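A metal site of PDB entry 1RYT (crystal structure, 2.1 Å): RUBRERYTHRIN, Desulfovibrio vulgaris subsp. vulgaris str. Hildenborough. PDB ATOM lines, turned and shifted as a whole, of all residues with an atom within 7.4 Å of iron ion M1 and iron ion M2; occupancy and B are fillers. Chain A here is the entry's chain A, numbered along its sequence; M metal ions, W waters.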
ATOM      1  N   ALA A  15     -14.272 -16.257  15.243  1.00  0.00           N
ATOM      2  CA  ALA A  15     -15.028 -16.205  16.492  1.00  0.00           C
ATOM      3  C   ALA A  15     -14.999 -14.749  17.002  1.00  0.00           C
ATOM      4  O   ALA A  15     -16.042 -14.170  17.359  1.00  0.00           O
ATOM      5  CB  ALA A  15     -14.427 -17.160  17.498  1.00  0.00           C
ATOM      6  N   GLY A  18     -17.501 -12.649  14.846  1.00  0.00           N
ATOM      7  CA  GLY A  18     -18.896 -12.913  15.147  1.00  0.00           C
ATOM      8  C   GLY A  18     -19.211 -12.362  16.522  1.00  0.00           C
ATOM      9  O   GLY A  18     -20.264 -11.734  16.713  1.00  0.00           O
ATOM     10  N   GLU A  19     -18.328 -12.566  17.493  1.00  0.00           N
ATOM     11  CA  GLU A  19     -18.594 -12.047  18.839  1.00  0.00           C
ATOM     12  C   GLU A  19     -18.660 -10.519  18.824  1.00  0.00           C
ATOM     13  O   GLU A  19     -19.491  -9.920  19.519  1.00  0.00           O
ATOM     14  CB  GLU A  19     -17.556 -12.552  19.867  1.00  0.00           C
ATOM     15  CG  GLU A  19     -17.533 -14.063  20.091  1.00  0.00           C
ATOM     16  CD  GLU A  19     -18.736 -14.601  20.874  1.00  0.00           C
ATOM     17  OE1 GLU A  19     -19.888 -14.442  20.434  1.00  0.00           O
ATOM     18  OE2 GLU A  19     -18.527 -15.228  21.932  1.00  0.00           O
ATOM     19  N   ALA A  22     -22.000  -9.558  17.553  1.00  0.00           N
ATOM     20  CA  ALA A  22     -23.031  -9.926  18.546  1.00  0.00           C
ATOM     21  C   ALA A  22     -23.137  -8.861  19.633  1.00  0.00           C
ATOM     22  O   ALA A  22     -24.234  -8.500  20.043  1.00  0.00           O
ATOM     23  CB  ALA A  22     -22.781 -11.320  19.146  1.00  0.00           C
ATOM     24  N   TYR A  26     -26.652  -7.091  20.366  1.00  0.00           N
ATOM     25  CA  TYR A  26     -27.272  -7.145  21.689  1.00  0.00           C
ATOM     26  C   TYR A  26     -27.502  -5.743  22.270  1.00  0.00           C
ATOM     27  O   TYR A  26     -28.535  -5.475  22.897  1.00  0.00           O
ATOM     28  CB  TYR A  26     -26.479  -8.047  22.670  1.00  0.00           C
ATOM     29  CG  TYR A  26     -26.455  -9.523  22.257  1.00  0.00           C
ATOM     30  CD1 TYR A  26     -27.475 -10.070  21.462  1.00  0.00           C
ATOM     31  CD2 TYR A  26     -25.390 -10.346  22.626  1.00  0.00           C
ATOM     32  CE1 TYR A  26     -27.425 -11.412  21.019  1.00  0.00           C
ATOM     33  CE2 TYR A  26     -25.327 -11.703  22.194  1.00  0.00           C
ATOM     34  CZ  TYR A  26     -26.343 -12.199  21.404  1.00  0.00           C
ATOM     35  OH  TYR A  26     -26.299 -13.526  20.987  1.00  0.00           O
ATOM     36  N   THR A  48     -25.332  -9.142  28.336  1.00  0.00           N
ATOM     37  CA  THR A  48     -24.871 -10.130  27.391  1.00  0.00           C
ATOM     38  C   THR A  48     -23.907  -9.515  26.384  1.00  0.00           C
ATOM     39  O   THR A  48     -22.897 -10.130  26.018  1.00  0.00           O
ATOM     40  CB  THR A  48     -26.047 -10.804  26.689  1.00  0.00           C
ATOM     41  OG1 THR A  48     -27.036 -11.144  27.662  1.00  0.00           O
ATOM     42  CG2 THR A  48     -25.602 -12.074  25.966  1.00  0.00           C
ATOM     43  N   GLN A  51     -20.679  -9.377  28.068  1.00  0.00           N
ATOM     44  CA  GLN A  51     -20.020 -10.652  28.218  1.00  0.00           C
ATOM     45  C   GLN A  51     -19.423 -11.088  26.896  1.00  0.00           C
ATOM     46  O   GLN A  51     -18.324 -11.637  26.894  1.00  0.00           O
ATOM     47  CB  GLN A  51     -21.006 -11.677  28.804  1.00  0.00           C
ATOM     48  CG  GLN A  51     -21.316 -11.323  30.244  1.00  0.00           C
ATOM     49  CD  GLN A  51     -22.334 -12.239  30.886  1.00  0.00           C
ATOM     50  OE1 GLN A  51     -23.104 -12.911  30.204  1.00  0.00           O
ATOM     51  NE2 GLN A  51     -22.334 -12.278  32.200  1.00  0.00           N
ATOM     52  N   GLU A  52     -20.074 -10.819  25.768  1.00  0.00           N
ATOM     53  CA  GLU A  52     -19.474 -11.180  24.473  1.00  0.00           C
ATOM     54  C   GLU A  52     -18.187 -10.379  24.242  1.00  0.00           C
ATOM     55  O   GLU A  52     -17.234 -10.861  23.622  1.00  0.00           O
ATOM     56  CB  GLU A  52     -20.410 -10.934  23.294  1.00  0.00           C
ATOM     57  CG  GLU A  52     -21.756 -11.616  23.340  1.00  0.00           C
ATOM     58  CD  GLU A  52     -21.707 -13.119  23.612  1.00  0.00           C
ATOM     59  OE1 GLU A  52     -20.801 -13.838  23.143  1.00  0.00           O
ATOM     60  OE2 GLU A  52     -22.620 -13.585  24.321  1.00  0.00           O
ATOM     61  N   HIS A  55     -15.576 -12.389  25.897  1.00  0.00           N
ATOM     62  CA  HIS A  55     -15.241 -13.627  25.213  1.00  0.00           C
ATOM     63  C   HIS A  55     -14.317 -13.171  24.067  1.00  0.00           C
ATOM     64  O   HIS A  55     -13.274 -13.771  23.820  1.00  0.00           O
ATOM     65  CB  HIS A  55     -16.485 -14.279  24.601  1.00  0.00           C
ATOM     66  CG  HIS A  55     -17.428 -14.868  25.609  1.00  0.00           C
ATOM     67  ND1 HIS A  55     -18.764 -15.088  25.331  1.00  0.00           N
ATOM     68  CD2 HIS A  55     -17.232 -15.296  26.876  1.00  0.00           C
ATOM     69  CE1 HIS A  55     -19.342 -15.624  26.390  1.00  0.00           C
ATOM     70  NE2 HIS A  55     -18.435 -15.751  27.342  1.00  0.00           N
ATOM     71  N   ALA A  56     -14.712 -12.080  23.397  1.00  0.00           N
ATOM     72  CA  ALA A  56     -13.929 -11.530  22.303  1.00  0.00           C
ATOM     73  C   ALA A  56     -12.510 -11.104  22.737  1.00  0.00           C
ATOM     74  O   ALA A  56     -11.538 -11.330  22.021  1.00  0.00           O
ATOM     75  CB  ALA A  56     -14.691 -10.384  21.646  1.00  0.00           C
ATOM     76  N   SER A  89     -31.722 -13.950  18.829  1.00  0.00           N
ATOM     77  CA  SER A  89     -30.533 -14.044  19.670  1.00  0.00           C
ATOM     78  C   SER A  89     -30.272 -15.468  20.146  1.00  0.00           C
ATOM     79  O   SER A  89     -29.170 -15.962  19.978  1.00  0.00           O
ATOM     80  CB  SER A  89     -30.664 -13.095  20.872  1.00  0.00           C
ATOM     81  OG  SER A  89     -30.684 -11.731  20.454  1.00  0.00           O
ATOM     82  N   GLY A  92     -28.837 -17.524  17.523  1.00  0.00           N
ATOM     83  CA  GLY A  92     -27.432 -17.270  17.267  1.00  0.00           C
ATOM     84  C   GLY A  92     -26.574 -17.917  18.331  1.00  0.00           C
ATOM     85  O   GLY A  92     -25.541 -18.532  18.042  1.00  0.00           O
ATOM     86  N   GLU A  93     -27.022 -17.782  19.575  1.00  0.00           N
ATOM     87  CA  GLU A  93     -26.343 -18.355  20.732  1.00  0.00           C
ATOM     88  C   GLU A  93     -26.322 -19.844  20.544  1.00  0.00           C
ATOM     89  O   GLU A  93     -25.301 -20.507  20.728  1.00  0.00           O
ATOM     90  CB  GLU A  93     -27.122 -18.017  22.000  1.00  0.00           C
ATOM     91  CG  GLU A  93     -27.109 -16.539  22.409  1.00  0.00           C
ATOM     92  CD  GLU A  93     -25.769 -16.084  22.987  1.00  0.00           C
ATOM     93  OE1 GLU A  93     -24.843 -16.920  23.042  1.00  0.00           O
ATOM     94  OE2 GLU A  93     -25.657 -14.915  23.396  1.00  0.00           O
ATOM     95  N   HIS A  94     -27.440 -20.368  20.060  1.00  0.00           N
ATOM     96  CA  HIS A  94     -27.581 -21.787  19.850  1.00  0.00           C
ATOM     97  C   HIS A  94     -26.534 -22.337  18.922  1.00  0.00           C
ATOM     98  O   HIS A  94     -25.945 -23.383  19.199  1.00  0.00           O
ATOM     99  CB  HIS A  94     -28.947 -22.128  19.291  1.00  0.00           C
ATOM    100  CG  HIS A  94     -29.163 -23.589  19.138  1.00  0.00           C
ATOM    101  ND1 HIS A  94     -29.558 -24.395  20.194  1.00  0.00           N
ATOM    102  CD2 HIS A  94     -29.009 -24.416  18.081  1.00  0.00           C
ATOM    103  CE1 HIS A  94     -29.640 -25.646  19.783  1.00  0.00           C
ATOM    104  NE2 HIS A  94     -29.315 -25.690  18.500  1.00  0.00           N
ATOM    105  N   GLU A  96     -23.657 -21.067  18.173  1.00  0.00           N
ATOM    106  CA  GLU A  96     -22.318 -20.938  18.727  1.00  0.00           C
ATOM    107  C   GLU A  96     -21.912 -22.098  19.624  1.00  0.00           C
ATOM    108  O   GLU A  96     -20.828 -22.667  19.463  1.00  0.00           O
ATOM    109  CB  GLU A  96     -22.175 -19.606  19.474  1.00  0.00           C
ATOM    110  CG  GLU A  96     -21.954 -18.387  18.589  1.00  0.00           C
ATOM    111  CD  GLU A  96     -21.758 -17.098  19.387  1.00  0.00           C
ATOM    112  OE1 GLU A  96     -20.900 -17.051  20.279  1.00  0.00           O
ATOM    113  OE2 GLU A  96     -22.463 -16.126  19.105  1.00  0.00           O
ATOM    114  N   TYR A  97     -22.779 -22.484  20.547  1.00  0.00           N
ATOM    115  CA  TYR A  97     -22.444 -23.554  21.467  1.00  0.00           C
ATOM    116  C   TYR A  97     -22.670 -24.946  20.907  1.00  0.00           C
ATOM    117  O   TYR A  97     -22.026 -25.895  21.317  1.00  0.00           O
ATOM    118  CB  TYR A  97     -23.105 -23.353  22.850  1.00  0.00           C
ATOM    119  CG  TYR A  97     -24.547 -23.815  23.024  1.00  0.00           C
ATOM    120  CD1 TYR A  97     -24.834 -25.141  23.311  1.00  0.00           C
ATOM    121  CD2 TYR A  97     -25.609 -22.918  22.935  1.00  0.00           C
ATOM    122  CE1 TYR A  97     -26.151 -25.576  23.510  1.00  0.00           C
ATOM    123  CE2 TYR A  97     -26.933 -23.331  23.142  1.00  0.00           C
ATOM    124  CZ  TYR A  97     -27.188 -24.663  23.429  1.00  0.00           C
ATOM    125  OH  TYR A  97     -28.492 -25.112  23.615  1.00  0.00           O
ATOM    126  N   MET A 100     -20.451 -23.921  16.185  1.00  0.00           N
ATOM    127  CA  MET A 100     -19.177 -23.208  16.067  1.00  0.00           C
ATOM    128  C   MET A 100     -18.102 -23.607  17.073  1.00  0.00           C
ATOM    129  O   MET A 100     -17.080 -24.193  16.704  1.00  0.00           O
ATOM    130  CB  MET A 100     -19.422 -21.705  16.123  1.00  0.00           C
ATOM    131  CG  MET A 100     -18.222 -20.894  15.661  1.00  0.00           C
ATOM    132  SD  MET A 100     -18.513 -19.141  15.837  1.00  0.00           S
ATOM    133  CE  MET A 100     -17.936 -18.927  17.450  1.00  0.00           C
ATOM    134  N   TYR A 101     -18.319 -23.301  18.348  1.00  0.00           N
ATOM    135  CA  TYR A 101     -17.335 -23.617  19.365  1.00  0.00           C
ATOM    136  C   TYR A 101     -16.858 -25.075  19.492  1.00  0.00           C
ATOM    137  O   TYR A 101     -15.653 -25.318  19.622  1.00  0.00           O
ATOM    138  CB  TYR A 101     -17.749 -23.022  20.714  1.00  0.00           C
ATOM    139  CG  TYR A 101     -17.535 -21.518  20.802  1.00  0.00           C
ATOM    140  CD1 TYR A 101     -16.249 -20.979  20.676  1.00  0.00           C
ATOM    141  CD2 TYR A 101     -18.606 -20.656  21.011  1.00  0.00           C
ATOM    142  CE1 TYR A 101     -16.035 -19.597  20.770  1.00  0.00           C
ATOM    143  CE2 TYR A 101     -18.407 -19.274  21.089  1.00  0.00           C
ATOM    144  CZ  TYR A 101     -17.118 -18.765  20.983  1.00  0.00           C
ATOM    145  OH  TYR A 101     -16.897 -17.401  21.150  1.00  0.00           O
ATOM    146  N   ILE A 123     -16.273 -21.309  26.721  1.00  0.00           N
ATOM    147  CA  ILE A 123     -17.127 -20.221  26.247  1.00  0.00           C
ATOM    148  C   ILE A 123     -18.506 -20.775  25.879  1.00  0.00           C
ATOM    149  O   ILE A 123     -19.532 -20.157  26.180  1.00  0.00           O
ATOM    150  CB  ILE A 123     -16.487 -19.486  25.028  1.00  0.00           C
ATOM    151  CG1 ILE A 123     -15.242 -18.712  25.479  1.00  0.00           C
ATOM    152  CG2 ILE A 123     -17.483 -18.543  24.372  1.00  0.00           C
ATOM    153  CD1 ILE A 123     -14.355 -18.238  24.326  1.00  0.00           C
ATOM    154  N   ALA A 126     -21.061 -20.851  28.600  1.00  0.00           N
ATOM    155  CA  ALA A 126     -21.690 -19.551  28.863  1.00  0.00           C
ATOM    156  C   ALA A 126     -22.721 -19.232  27.773  1.00  0.00           C
ATOM    157  O   ALA A 126     -23.767 -18.621  28.037  1.00  0.00           O
ATOM    158  CB  ALA A 126     -20.620 -18.468  28.898  1.00  0.00           C
ATOM    159  N   GLU A 127     -22.418 -19.668  26.564  1.00  0.00           N
ATOM    160  CA  GLU A 127     -23.290 -19.449  25.429  1.00  0.00           C
ATOM    161  C   GLU A 127     -24.570 -20.251  25.566  1.00  0.00           C
ATOM    162  O   GLU A 127     -25.596 -19.901  24.999  1.00  0.00           O
ATOM    163  CB  GLU A 127     -22.567 -19.740  24.118  1.00  0.00           C
ATOM    164  CG  GLU A 127     -21.208 -19.070  23.986  1.00  0.00           C
ATOM    165  CD  GLU A 127     -21.263 -17.553  23.812  1.00  0.00           C
ATOM    166  OE1 GLU A 127     -22.105 -16.863  24.423  1.00  0.00           O
ATOM    167  OE2 GLU A 127     -20.409 -17.028  23.077  1.00  0.00           O
ATOM    168  N   GLU A 128     -24.517 -21.334  26.334  1.00  0.00           N
ATOM    169  CA  GLU A 128     -25.710 -22.143  26.555  1.00  0.00           C
ATOM    170  C   GLU A 128     -26.677 -21.460  27.539  1.00  0.00           C
ATOM    171  O   GLU A 128     -27.888 -21.508  27.349  1.00  0.00           O
ATOM    172  CB  GLU A 128     -25.335 -23.549  27.023  1.00  0.00           C
ATOM    173  CG  GLU A 128     -26.521 -24.420  27.357  1.00  0.00           C
ATOM    174  CD  GLU A 128     -26.177 -25.904  27.300  1.00  0.00           C
ATOM    175  OE1 GLU A 128     -24.984 -26.257  27.474  1.00  0.00           O
ATOM    176  OE2 GLU A 128     -27.100 -26.712  27.054  1.00  0.00           O
ATOM    177  N   PHE A 129     -26.143 -20.803  28.574  1.00  0.00           N
ATOM    178  CA  PHE A 129     -27.015 -20.090  29.524  1.00  0.00           C
ATOM    179  C   PHE A 129     -27.624 -18.827  28.852  1.00  0.00           C
ATOM    180  O   PHE A 129     -28.792 -18.500  29.086  1.00  0.00           O
ATOM    181  CB  PHE A 129     -26.277 -19.760  30.848  1.00  0.00           C
ATOM    182  CG  PHE A 129     -27.154 -19.095  31.900  1.00  0.00           C
ATOM    183  CD1 PHE A 129     -28.304 -19.734  32.386  1.00  0.00           C
ATOM    184  CD2 PHE A 129     -26.887 -17.795  32.347  1.00  0.00           C
ATOM    185  CE1 PHE A 129     -29.182 -19.090  33.295  1.00  0.00           C
ATOM    186  CE2 PHE A 129     -27.759 -17.143  33.252  1.00  0.00           C
ATOM    187  CZ  PHE A 129     -28.906 -17.793  33.721  1.00  0.00           C
ATOM    188  N   HIS A 130     -26.878 -18.154  27.986  1.00  0.00           N
ATOM    189  CA  HIS A 130     -27.406 -16.970  27.298  1.00  0.00           C
ATOM    190  C   HIS A 130     -28.635 -17.317  26.510  1.00  0.00           C
ATOM    191  O   HIS A 130     -29.590 -16.568  26.527  1.00  0.00           O
ATOM    192  CB  HIS A 130     -26.391 -16.392  26.302  1.00  0.00           C
ATOM    193  CG  HIS A 130     -25.199 -15.761  26.962  1.00  0.00           C
ATOM    194  ND1 HIS A 130     -24.058 -15.445  26.269  1.00  0.00           N
ATOM    195  CD2 HIS A 130     -24.993 -15.336  28.236  1.00  0.00           C
ATOM    196  CE1 HIS A 130     -23.199 -14.848  27.079  1.00  0.00           C
ATOM    197  NE2 HIS A 130     -23.740 -14.770  28.278  1.00  0.00           N
ATOM    198  N   GLU A 131     -28.580 -18.429  25.778  1.00  0.00           N
ATOM    199  CA  GLU A 131     -29.713 -18.894  24.965  1.00  0.00           C
ATOM    200  C   GLU A 131     -30.902 -19.225  25.826  1.00  0.00           C
ATOM    201  O   GLU A 131     -32.016 -18.840  25.530  1.00  0.00           O
ATOM    202  CB  GLU A 131     -29.371 -20.151  24.199  1.00  0.00           C
ATOM    203  CG  GLU A 131     -30.532 -20.582  23.346  1.00  0.00           C
ATOM    204  CD  GLU A 131     -30.548 -22.070  23.040  1.00  0.00           C
ATOM    205  OE1 GLU A 131     -30.081 -22.867  23.879  1.00  0.00           O
ATOM    206  OE2 GLU A 131     -31.065 -22.430  21.966  1.00  0.00           O
ATOM    207  N   PHE A 134     -32.563 -16.127  27.090  1.00  0.00           N
ATOM    208  CA  PHE A 134     -33.298 -15.423  26.030  1.00  0.00           C
ATOM    209  C   PHE A 134     -34.602 -16.117  25.696  1.00  0.00           C
ATOM    210  O   PHE A 134     -35.610 -15.470  25.344  1.00  0.00           O
ATOM    211  CB  PHE A 134     -32.445 -15.285  24.744  1.00  0.00           C
ATOM    212  CG  PHE A 134     -31.350 -14.250  24.838  1.00  0.00           C
ATOM    213  CD1 PHE A 134     -31.542 -13.053  25.557  1.00  0.00           C
ATOM    214  CD2 PHE A 134     -30.149 -14.443  24.178  1.00  0.00           C
ATOM    215  CE1 PHE A 134     -30.554 -12.093  25.602  1.00  0.00           C
ATOM    216  CE2 PHE A 134     -29.135 -13.473  24.223  1.00  0.00           C
ATOM    217  CZ  PHE A 134     -29.347 -12.302  24.941  1.00  0.00           C
HETATM  218 FE    FE M   1     -21.010 -15.525  21.833  1.00  0.00          FE
HETATM  219 FE    FE M   2     -23.479 -15.465  23.838  1.00  0.00          FE
HETATM  220  O   HOH W   1     -22.916 -15.302  21.733  1.00  0.00           O
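Iron ion M2 is bound by the side-chain carboxylate (OE1) of Glu 127 (2.0 Å), the side-chain carboxylate (OE2) of Glu 52 (2.1 Å), the side-chain carboxylate (OE1) of Glu 93 (2.1 Å), water W1 (2.2 Å), the side-chain carboxylate (OE2) of Glu 93 (2.3 Å) and a ring nitrogen (ND1) of His 130 (2.5 Å).
Iron ion M2 has six donor atoms within binding distance.
A ring nitrogen (ND1) of His 55 lies close to the side-chain carboxylate (OE2) of Glu 127, at 3.4 Å.
The side-chain carboxylate (OE2) of Glu 19 sits close to a ring nitrogen (ND1) of His 55 (3.4 Å).
OE2 of Glu 19 sits close to OH of Tyr 101.
The side-chain carboxylate (OE1) of Glu 52 sits close to a ring nitrogen (ND1) of His 55.
OH of Tyr 26 sits close to OE2 of Glu 93, at 2.9 Å.
O of Glu 96 is in hydrogen-bond range of N of Tyr 101 (2.8 Å).
OE1 of Gln 51 is in hydrogen-bond range of NE2 of His 130, at 2.8 Å.
Iron ion M1 is bound by water W1.
Iron ion M1 is bound by OE2 of Glu 127.
Iron ion M1 is bound by OE1 of Glu 19, 2.1 Å away.
Iron ion M1 is bound by OE1 of Glu 52.
Iron ion M1 is bound by OE1 of Glu 96 (2.2 Å).
Iron ion M1 is bound by OE2 of Glu 19, at 2.5 Å.
Within 4 Å of iron ion M1: Glu 19, Glu 52, Glu 96 and Glu 127.
Within 4 Å of iron ion M2: Glu 52, Glu 93, Glu 127 and His 130.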
